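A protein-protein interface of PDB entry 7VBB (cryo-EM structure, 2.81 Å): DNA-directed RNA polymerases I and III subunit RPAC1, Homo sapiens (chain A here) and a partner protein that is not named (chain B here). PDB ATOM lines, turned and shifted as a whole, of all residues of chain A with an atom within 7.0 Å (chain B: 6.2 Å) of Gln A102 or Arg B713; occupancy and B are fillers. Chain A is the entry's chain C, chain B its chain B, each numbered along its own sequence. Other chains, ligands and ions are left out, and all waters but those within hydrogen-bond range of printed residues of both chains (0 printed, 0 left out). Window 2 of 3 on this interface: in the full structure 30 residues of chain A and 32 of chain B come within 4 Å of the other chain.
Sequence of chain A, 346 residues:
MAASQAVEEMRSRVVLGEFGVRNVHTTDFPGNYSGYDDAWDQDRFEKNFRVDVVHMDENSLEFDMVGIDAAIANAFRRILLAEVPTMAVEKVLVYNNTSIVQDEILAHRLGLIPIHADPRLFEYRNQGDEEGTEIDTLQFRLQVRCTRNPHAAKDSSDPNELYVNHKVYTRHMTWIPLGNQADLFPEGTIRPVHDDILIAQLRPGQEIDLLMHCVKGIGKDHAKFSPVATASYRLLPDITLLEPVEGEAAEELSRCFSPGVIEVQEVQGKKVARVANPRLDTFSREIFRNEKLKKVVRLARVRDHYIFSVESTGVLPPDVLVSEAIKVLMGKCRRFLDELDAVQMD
The guanidinium group (NE) of Arg B872 is in salt-bridge range of the side-chain carboxylate (OE1) of Glu A104 (3.3 Å).
Of the 16 printed residues of chain B, 3 touch a printed residue of chain A.
Printed residues of chain A that touch a printed residue of chain B: Gln A102, Asp A103, Glu A104 and Ile A105.
Hydrophobic or aromatic side chains of chain A within 4 Å of the printed part of chain B: Ile A105.
Among the printed residues, pairs that only touch across the chains: Gln A102 with Arg B872 (3.3 Å), Ile A105 with Gln B715 (3.6 Å), Gln A102 with Gln B715 (3.6 Å), Gln A102 with Arg B713 (3.97 Å) and Asp A103 with Arg B872 (3.996 Å).
The backbone carbonyl oxygen (O) of Arg B713 sits at hydrogen-bond distance from the backbone NH (N) of Ser B772 (2.9 Å).
O of His B770 sits at hydrogen-bond distance from N of Gln B715, 3.1 Å away.
The guanidinium group of Arg B713 lies within hydrogen-bond range of the side-chain hydroxyl of Tyr B774 (3.2 Å).
OD1 of Asp A103 sits at hydrogen-bond distance from ND2 of Asn A97 (2.6 Å).
The backbone carbonyl oxygen (O) of Ile A100 lies close to the side-chain amide oxygen (OE1) of Gln A102 (2.9 Å).
Gln A102 touches just these residues of chain B: Arg B713, Gln B715 and Arg B872.
Of the printed residues of chain A, Arg B872 touches Gln A102 (3.3 Å), Asp A103 (3.996 Å) and Glu A104 (3.3 Å).
Printed residues of chain B within 4 Å of Asp A103: Arg B872 (3.996 Å).
Of the printed residues of chain B, Ile A105 touches Gln B715 (3.6 Å).
Of the printed residues of chain A, Gln B715 touches Gln A102 (3.6 Å) and Ile A105 (3.6 Å).
Leu A106 touches none of the printed residues of chain B.
The nearest residue of chain B that does not touch Gln A102 is Tyr B774 (4.05 Å).
The nearest printed residue of chain B that does not touch Ile A105 is Ser B772 (4.6 Å).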
ATOM      1  N   ASN A  97      35.712   8.047 -20.612  1.00  0.00           N
ATOM      2  CA  ASN A  97      35.870   7.457 -19.284  1.00  0.00           C
ATOM      3  C   ASN A  97      36.006   5.952 -19.470  1.00  0.00           C
ATOM      4  O   ASN A  97      35.002   5.247 -19.601  1.00  0.00           O
ATOM      5  CB  ASN A  97      34.688   7.794 -18.383  1.00  0.00           C
ATOM      6  CG  ASN A  97      34.805   7.171 -17.007  1.00  0.00           C
ATOM      7  OD1 ASN A  97      35.751   6.443 -16.721  1.00  0.00           O
ATOM      8  ND2 ASN A  97      33.832   7.446 -16.152  1.00  0.00           N
ATOM      9  N   SER A  99      37.255   3.910 -17.188  1.00  0.00           N
ATOM     10  CA  SER A  99      37.494   3.375 -15.861  1.00  0.00           C
ATOM     11  C   SER A  99      36.499   2.265 -15.537  1.00  0.00           C
ATOM     12  O   SER A  99      35.519   2.038 -16.252  1.00  0.00           O
ATOM     13  CB  SER A  99      37.394   4.482 -14.814  1.00  0.00           C
ATOM     14  OG  SER A  99      38.560   5.281 -14.802  1.00  0.00           O
ATOM     15  N   ILE A 100      36.770   1.559 -14.438  1.00  0.00           N
ATOM     16  CA  ILE A 100      35.810   0.588 -13.928  1.00  0.00           C
ATOM     17  C   ILE A 100      34.631   1.294 -13.275  1.00  0.00           C
ATOM     18  O   ILE A 100      33.507   0.780 -13.283  1.00  0.00           O
ATOM     19  CB  ILE A 100      36.498  -0.382 -12.950  1.00  0.00           C
ATOM     20  CG1 ILE A 100      37.397  -1.349 -13.712  1.00  0.00           C
ATOM     21  CG2 ILE A 100      35.470  -1.153 -12.150  1.00  0.00           C
ATOM     22  CD1 ILE A 100      36.674  -2.118 -14.788  1.00  0.00           C
ATOM     23  N   VAL A 101      34.863   2.475 -12.702  1.00  0.00           N
ATOM     24  CA  VAL A 101      33.786   3.240 -12.087  1.00  0.00           C
ATOM     25  C   VAL A 101      32.904   3.836 -13.176  1.00  0.00           C
ATOM     26  O   VAL A 101      33.396   4.455 -14.128  1.00  0.00           O
ATOM     27  CB  VAL A 101      34.359   4.331 -11.172  1.00  0.00           C
ATOM     28  CG1 VAL A 101      33.269   4.902 -10.288  1.00  0.00           C
ATOM     29  CG2 VAL A 101      35.488   3.769 -10.326  1.00  0.00           C
ATOM     30  N   GLN A 102      31.595   3.657 -13.036  1.00  0.00           N
ATOM     31  CA  GLN A 102      30.652   4.093 -14.052  1.00  0.00           C
ATOM     32  C   GLN A 102      30.659   5.617 -14.167  1.00  0.00           C
ATOM     33  O   GLN A 102      31.321   6.327 -13.409  1.00  0.00           O
ATOM     34  CB  GLN A 102      29.252   3.584 -13.723  1.00  0.00           C
ATOM     35  CG  GLN A 102      29.018   2.139 -14.103  1.00  0.00           C
ATOM     36  CD  GLN A 102      29.756   1.177 -13.204  1.00  0.00           C
ATOM     37  OE1 GLN A 102      30.677   0.488 -13.639  1.00  0.00           O
ATOM     38  NE2 GLN A 102      29.351   1.116 -11.942  1.00  0.00           N
ATOM     39  N   ASP A 103      29.902   6.124 -15.140  1.00  0.00           N
ATOM     40  CA  ASP A 103      29.811   7.565 -15.344  1.00  0.00           C
ATOM     41  C   ASP A 103      28.865   8.207 -14.338  1.00  0.00           C
ATOM     42  O   ASP A 103      29.187   9.240 -13.742  1.00  0.00           O
ATOM     43  CB  ASP A 103      29.352   7.864 -16.770  1.00  0.00           C
ATOM     44  CG  ASP A 103      30.453   7.667 -17.788  1.00  0.00           C
ATOM     45  OD1 ASP A 103      31.627   7.910 -17.444  1.00  0.00           O
ATOM     46  OD2 ASP A 103      30.145   7.271 -18.932  1.00  0.00           O
ATOM     47  N   GLU A 104      27.693   7.604 -14.133  1.00  0.00           N
ATOM     48  CA  GLU A 104      26.755   8.133 -13.152  1.00  0.00           C
ATOM     49  C   GLU A 104      27.282   7.981 -11.733  1.00  0.00           C
ATOM     50  O   GLU A 104      27.095   8.876 -10.902  1.00  0.00           O
ATOM     51  CB  GLU A 104      25.405   7.436 -13.300  1.00  0.00           C
ATOM     52  CG  GLU A 104      25.498   5.919 -13.306  1.00  0.00           C
ATOM     53  CD  GLU A 104      25.552   5.341 -14.706  1.00  0.00           C
ATOM     54  OE1 GLU A 104      24.732   4.451 -15.016  1.00  0.00           O
ATOM     55  OE2 GLU A 104      26.415   5.772 -15.498  1.00  0.00           O
ATOM     56  N   ILE A 105      27.961   6.869 -11.443  1.00  0.00           N
ATOM     57  CA  ILE A 105      28.539   6.674 -10.118  1.00  0.00           C
ATOM     58  C   ILE A 105      29.711   7.620  -9.900  1.00  0.00           C
ATOM     59  O   ILE A 105      29.929   8.112  -8.788  1.00  0.00           O
ATOM     60  CB  ILE A 105      28.953   5.206  -9.933  1.00  0.00           C
ATOM     61  CG1 ILE A 105      27.711   4.318  -9.872  1.00  0.00           C
ATOM     62  CG2 ILE A 105      29.811   5.047  -8.692  1.00  0.00           C
ATOM     63  CD1 ILE A 105      27.215   3.874 -11.220  1.00  0.00           C
ATOM     64  N   LEU A 106      30.477   7.899 -10.954  1.00  0.00           N
ATOM     65  CA  LEU A 106      31.538   8.891 -10.842  1.00  0.00           C
ATOM     66  C   LEU A 106      30.968  10.278 -10.587  1.00  0.00           C
ATOM     67  O   LEU A 106      31.495  11.029  -9.761  1.00  0.00           O
ATOM     68  CB  LEU A 106      32.395   8.887 -12.105  1.00  0.00           C
ATOM     69  CG  LEU A 106      33.838   9.350 -11.939  1.00  0.00           C
ATOM     70  CD1 LEU A 106      34.515   8.571 -10.828  1.00  0.00           C
ATOM     71  CD2 LEU A 106      34.586   9.182 -13.241  1.00  0.00           C
ATOM     72  N   ALA A 107      29.890  10.638 -11.286  1.00  0.00           N
ATOM     73  CA  ALA A 107      29.252  11.926 -11.042  1.00  0.00           C
ATOM     74  C   ALA A 107      28.748  12.027  -9.608  1.00  0.00           C
ATOM     75  O   ALA A 107      28.949  13.048  -8.938  1.00  0.00           O
ATOM     76  CB  ALA A 107      28.110  12.139 -12.031  1.00  0.00           C
ATOM     77  N   MET B 696      18.955  -7.635  -4.478  1.00  0.00           N
ATOM     78  CA  MET B 696      19.896  -6.904  -5.312  1.00  0.00           C
ATOM     79  C   MET B 696      21.242  -6.883  -4.604  1.00  0.00           C
ATOM     80  O   MET B 696      21.368  -6.311  -3.517  1.00  0.00           O
ATOM     81  CB  MET B 696      19.386  -5.489  -5.555  1.00  0.00           C
ATOM     82  CG  MET B 696      19.984  -4.785  -6.746  1.00  0.00           C
ATOM     83  SD  MET B 696      19.162  -3.211  -7.024  1.00  0.00           S
ATOM     84  CE  MET B 696      19.824  -2.739  -8.613  1.00  0.00           C
ATOM     85  N   GLY B 697      22.243  -7.519  -5.200  1.00  0.00           N
ATOM     86  CA  GLY B 697      23.544  -7.595  -4.571  1.00  0.00           C
ATOM     87  C   GLY B 697      24.682  -7.444  -5.554  1.00  0.00           C
ATOM     88  O   GLY B 697      24.573  -6.704  -6.533  1.00  0.00           O
ATOM     89  N   PHE B 698      25.789  -8.137  -5.297  1.00  0.00           N
ATOM     90  CA  PHE B 698      26.903  -8.185  -6.228  1.00  0.00           C
ATOM     91  C   PHE B 698      26.898  -9.559  -6.882  1.00  0.00           C
ATOM     92  O   PHE B 698      27.332 -10.537  -6.259  1.00  0.00           O
ATOM     93  CB  PHE B 698      28.226  -7.930  -5.503  1.00  0.00           C
ATOM     94  CG  PHE B 698      29.311  -7.409  -6.392  1.00  0.00           C
ATOM     95  CD1 PHE B 698      29.238  -6.130  -6.909  1.00  0.00           C
ATOM     96  CD2 PHE B 698      30.403  -8.191  -6.710  1.00  0.00           C
ATOM     97  CE1 PHE B 698      30.229  -5.644  -7.728  1.00  0.00           C
ATOM     98  CE2 PHE B 698      31.397  -7.706  -7.531  1.00  0.00           C
ATOM     99  CZ  PHE B 698      31.309  -6.432  -8.040  1.00  0.00           C
ATOM    100  N   PRO B 699      26.416  -9.694  -8.114  1.00  0.00           N
ATOM    101  CA  PRO B 699      26.134 -11.031  -8.650  1.00  0.00           C
ATOM    102  C   PRO B 699      27.358 -11.742  -9.197  1.00  0.00           C
ATOM    103  O   PRO B 699      27.409 -12.975  -9.190  1.00  0.00           O
ATOM    104  CB  PRO B 699      25.111 -10.748  -9.756  1.00  0.00           C
ATOM    105  CG  PRO B 699      25.340  -9.326 -10.155  1.00  0.00           C
ATOM    106  CD  PRO B 699      26.163  -8.637  -9.103  1.00  0.00           C
ATOM    107  N   TYR B 703      31.742  -8.449 -15.699  1.00  0.00           N
ATOM    108  CA  TYR B 703      30.921  -7.704 -16.635  1.00  0.00           C
ATOM    109  C   TYR B 703      31.720  -7.506 -17.912  1.00  0.00           C
ATOM    110  O   TYR B 703      32.918  -7.799 -17.967  1.00  0.00           O
ATOM    111  CB  TYR B 703      30.506  -6.362 -16.037  1.00  0.00           C
ATOM    112  CG  TYR B 703      29.713  -6.518 -14.766  1.00  0.00           C
ATOM    113  CD1 TYR B 703      28.356  -6.790 -14.804  1.00  0.00           C
ATOM    114  CD2 TYR B 703      30.329  -6.433 -13.527  1.00  0.00           C
ATOM    115  CE1 TYR B 703      27.630  -6.950 -13.642  1.00  0.00           C
ATOM    116  CE2 TYR B 703      29.612  -6.598 -12.362  1.00  0.00           C
ATOM    117  CZ  TYR B 703      28.263  -6.855 -12.424  1.00  0.00           C
ATOM    118  OH  TYR B 703      27.550  -7.017 -11.263  1.00  0.00           O
ATOM    119  N   LEU B 711      20.492  -8.026 -15.054  1.00  0.00           N
ATOM    120  CA  LEU B 711      21.558  -8.298 -14.095  1.00  0.00           C
ATOM    121  C   LEU B 711      21.601  -7.152 -13.095  1.00  0.00           C
ATOM    122  O   LEU B 711      22.136  -6.086 -13.400  1.00  0.00           O
ATOM    123  CB  LEU B 711      22.889  -8.473 -14.812  1.00  0.00           C
ATOM    124  CG  LEU B 711      24.041  -9.021 -13.983  1.00  0.00           C
ATOM    125  CD1 LEU B 711      25.019  -9.760 -14.870  1.00  0.00           C
ATOM    126  CD2 LEU B 711      24.730  -7.888 -13.268  1.00  0.00           C
ATOM    127  N   TYR B 712      21.052  -7.379 -11.904  1.00  0.00           N
ATOM    128  CA  TYR B 712      20.935  -6.349 -10.879  1.00  0.00           C
ATOM    129  C   TYR B 712      22.224  -6.260 -10.075  1.00  0.00           C
ATOM    130  O   TYR B 712      22.727  -7.275  -9.590  1.00  0.00           O
ATOM    131  CB  TYR B 712      19.764  -6.651  -9.946  1.00  0.00           C
ATOM    132  CG  TYR B 712      18.448  -6.810 -10.659  1.00  0.00           C
ATOM    133  CD1 TYR B 712      18.079  -8.026 -11.212  1.00  0.00           C
ATOM    134  CD2 TYR B 712      17.575  -5.744 -10.784  1.00  0.00           C
ATOM    135  CE1 TYR B 712      16.879  -8.172 -11.869  1.00  0.00           C
ATOM    136  CE2 TYR B 712      16.376  -5.880 -11.435  1.00  0.00           C
ATOM    137  CZ  TYR B 712      16.030  -7.093 -11.977  1.00  0.00           C
ATOM    138  OH  TYR B 712      14.824  -7.216 -12.628  1.00  0.00           O
ATOM    139  N   ARG B 713      22.741  -5.045  -9.917  1.00  0.00           N
ATOM    140  CA  ARG B 713      23.994  -4.824  -9.211  1.00  0.00           C
ATOM    141  C   ARG B 713      23.814  -3.747  -8.153  1.00  0.00           C
ATOM    142  O   ARG B 713      23.250  -2.686  -8.432  1.00  0.00           O
ATOM    143  CB  ARG B 713      25.104  -4.419 -10.179  1.00  0.00           C
ATOM    144  CG  ARG B 713      26.418  -4.102  -9.506  1.00  0.00           C
ATOM    145  CD  ARG B 713      27.395  -3.526 -10.499  1.00  0.00           C
ATOM    146  NE  ARG B 713      28.672  -3.199  -9.882  1.00  0.00           N
ATOM    147  CZ  ARG B 713      29.777  -2.929 -10.564  1.00  0.00           C
ATOM    148  NH1 ARG B 713      29.761  -2.950 -11.888  1.00  0.00           N
ATOM    149  NH2 ARG B 713      30.901  -2.644  -9.924  1.00  0.00           N
ATOM    150  N   LEU B 714      24.295  -4.021  -6.947  1.00  0.00           N
ATOM    151  CA  LEU B 714      24.334  -3.035  -5.877  1.00  0.00           C
ATOM    152  C   LEU B 714      25.714  -2.392  -5.828  1.00  0.00           C
ATOM    153  O   LEU B 714      26.733  -3.085  -5.882  1.00  0.00           O
ATOM    154  CB  LEU B 714      24.006  -3.695  -4.540  1.00  0.00           C
ATOM    155  CG  LEU B 714      23.836  -2.814  -3.308  1.00  0.00           C
ATOM    156  CD1 LEU B 714      22.418  -2.297  -3.222  1.00  0.00           C
ATOM    157  CD2 LEU B 714      24.189  -3.617  -2.079  1.00  0.00           C
ATOM    158  N   GLN B 715      25.744  -1.065  -5.716  1.00  0.00           N
ATOM    159  CA  GLN B 715      27.003  -0.346  -5.893  1.00  0.00           C
ATOM    160  C   GLN B 715      27.998  -0.667  -4.784  1.00  0.00           C
ATOM    161  O   GLN B 715      29.064  -1.237  -5.038  1.00  0.00           O
ATOM    162  CB  GLN B 715      26.748   1.158  -5.972  1.00  0.00           C
ATOM    163  CG  GLN B 715      26.187   1.594  -7.306  1.00  0.00           C
ATOM    164  CD  GLN B 715      26.938   0.974  -8.464  1.00  0.00           C
ATOM    165  OE1 GLN B 715      28.166   1.026  -8.522  1.00  0.00           O
ATOM    166  NE2 GLN B 715      26.202   0.369  -9.389  1.00  0.00           N
ATOM    167  N   HIS B 770      22.265   2.462  -3.389  1.00  0.00           N
ATOM    168  CA  HIS B 770      22.151   2.753  -4.809  1.00  0.00           C
ATOM    169  C   HIS B 770      22.442   1.497  -5.621  1.00  0.00           C
ATOM    170  O   HIS B 770      23.154   0.597  -5.176  1.00  0.00           O
ATOM    171  CB  HIS B 770      23.109   3.875  -5.197  1.00  0.00           C
ATOM    172  CG  HIS B 770      22.662   5.231  -4.748  1.00  0.00           C
ATOM    173  ND1 HIS B 770      23.429   6.361  -4.925  1.00  0.00           N
ATOM    174  CD2 HIS B 770      21.526   5.639  -4.137  1.00  0.00           C
ATOM    175  CE1 HIS B 770      22.786   7.408  -4.439  1.00  0.00           C
ATOM    176  NE2 HIS B 770      21.630   6.998  -3.954  1.00  0.00           N
ATOM    177  N   GLY B 771      21.882   1.436  -6.824  1.00  0.00           N
ATOM    178  CA  GLY B 771      22.000   0.226  -7.610  1.00  0.00           C
ATOM    179  C   GLY B 771      21.862   0.500  -9.091  1.00  0.00           C
ATOM    180  O   GLY B 771      21.768   1.647  -9.529  1.00  0.00           O
ATOM    181  N   SER B 772      21.858  -0.584  -9.861  1.00  0.00           N
ATOM    182  CA  SER B 772      21.768  -0.493 -11.311  1.00  0.00           C
ATOM    183  C   SER B 772      21.283  -1.822 -11.871  1.00  0.00           C
ATOM    184  O   SER B 772      21.312  -2.855 -11.200  1.00  0.00           O
ATOM    185  CB  SER B 772      23.116  -0.121 -11.934  1.00  0.00           C
ATOM    186  OG  SER B 772      23.538   1.166 -11.526  1.00  0.00           O
ATOM    187  N   VAL B 773      20.838  -1.778 -13.121  1.00  0.00           N
ATOM    188  CA  VAL B 773      20.441  -2.966 -13.865  1.00  0.00           C
ATOM    189  C   VAL B 773      21.146  -2.937 -15.211  1.00  0.00           C
ATOM    190  O   VAL B 773      21.312  -1.874 -15.814  1.00  0.00           O
ATOM    191  CB  VAL B 773      18.913  -3.042 -14.050  1.00  0.00           C
ATOM    192  CG1 VAL B 773      18.521  -4.374 -14.644  1.00  0.00           C
ATOM    193  CG2 VAL B 773      18.215  -2.829 -12.727  1.00  0.00           C
ATOM    194  N   TYR B 774      21.567  -4.104 -15.680  1.00  0.00           N
ATOM    195  CA  TYR B 774      22.220  -4.242 -16.977  1.00  0.00           C
ATOM    196  C   TYR B 774      21.291  -5.023 -17.892  1.00  0.00           C
ATOM    197  O   TYR B 774      21.079  -6.222 -17.693  1.00  0.00           O
ATOM    198  CB  TYR B 774      23.568  -4.946 -16.843  1.00  0.00           C
ATOM    199  CG  TYR B 774      24.593  -4.170 -16.055  1.00  0.00           C
ATOM    200  CD1 TYR B 774      24.528  -4.106 -14.674  1.00  0.00           C
ATOM    201  CD2 TYR B 774      25.630  -3.511 -16.693  1.00  0.00           C
ATOM    202  CE1 TYR B 774      25.462  -3.403 -13.950  1.00  0.00           C
ATOM    203  CE2 TYR B 774      26.569  -2.806 -15.979  1.00  0.00           C
ATOM    204  CZ  TYR B 774      26.481  -2.755 -14.606  1.00  0.00           C
ATOM    205  OH  TYR B 774      27.416  -2.053 -13.886  1.00  0.00           O
ATOM    206  N   ARG B 872      22.719   0.307 -19.402  1.00  0.00           N
ATOM    207  CA  ARG B 872      22.798   0.434 -17.955  1.00  0.00           C
ATOM    208  C   ARG B 872      21.678   1.357 -17.499  1.00  0.00           C
ATOM    209  O   ARG B 872      21.558   2.481 -17.995  1.00  0.00           O
ATOM    210  CB  ARG B 872      24.160   0.979 -17.532  1.00  0.00           C
ATOM    211  CG  ARG B 872      24.599   0.581 -16.143  1.00  0.00           C
ATOM    212  CD  ARG B 872      26.101   0.727 -16.009  1.00  0.00           C
ATOM    213  NE  ARG B 872      26.548   2.043 -16.450  1.00  0.00           N
ATOM    214  CZ  ARG B 872      27.676   2.265 -17.112  1.00  0.00           C
ATOM    215  NH1 ARG B 872      28.478   1.255 -17.414  1.00  0.00           N
ATOM    216  NH2 ARG B 872      28.003   3.496 -17.475  1.00  0.00           N
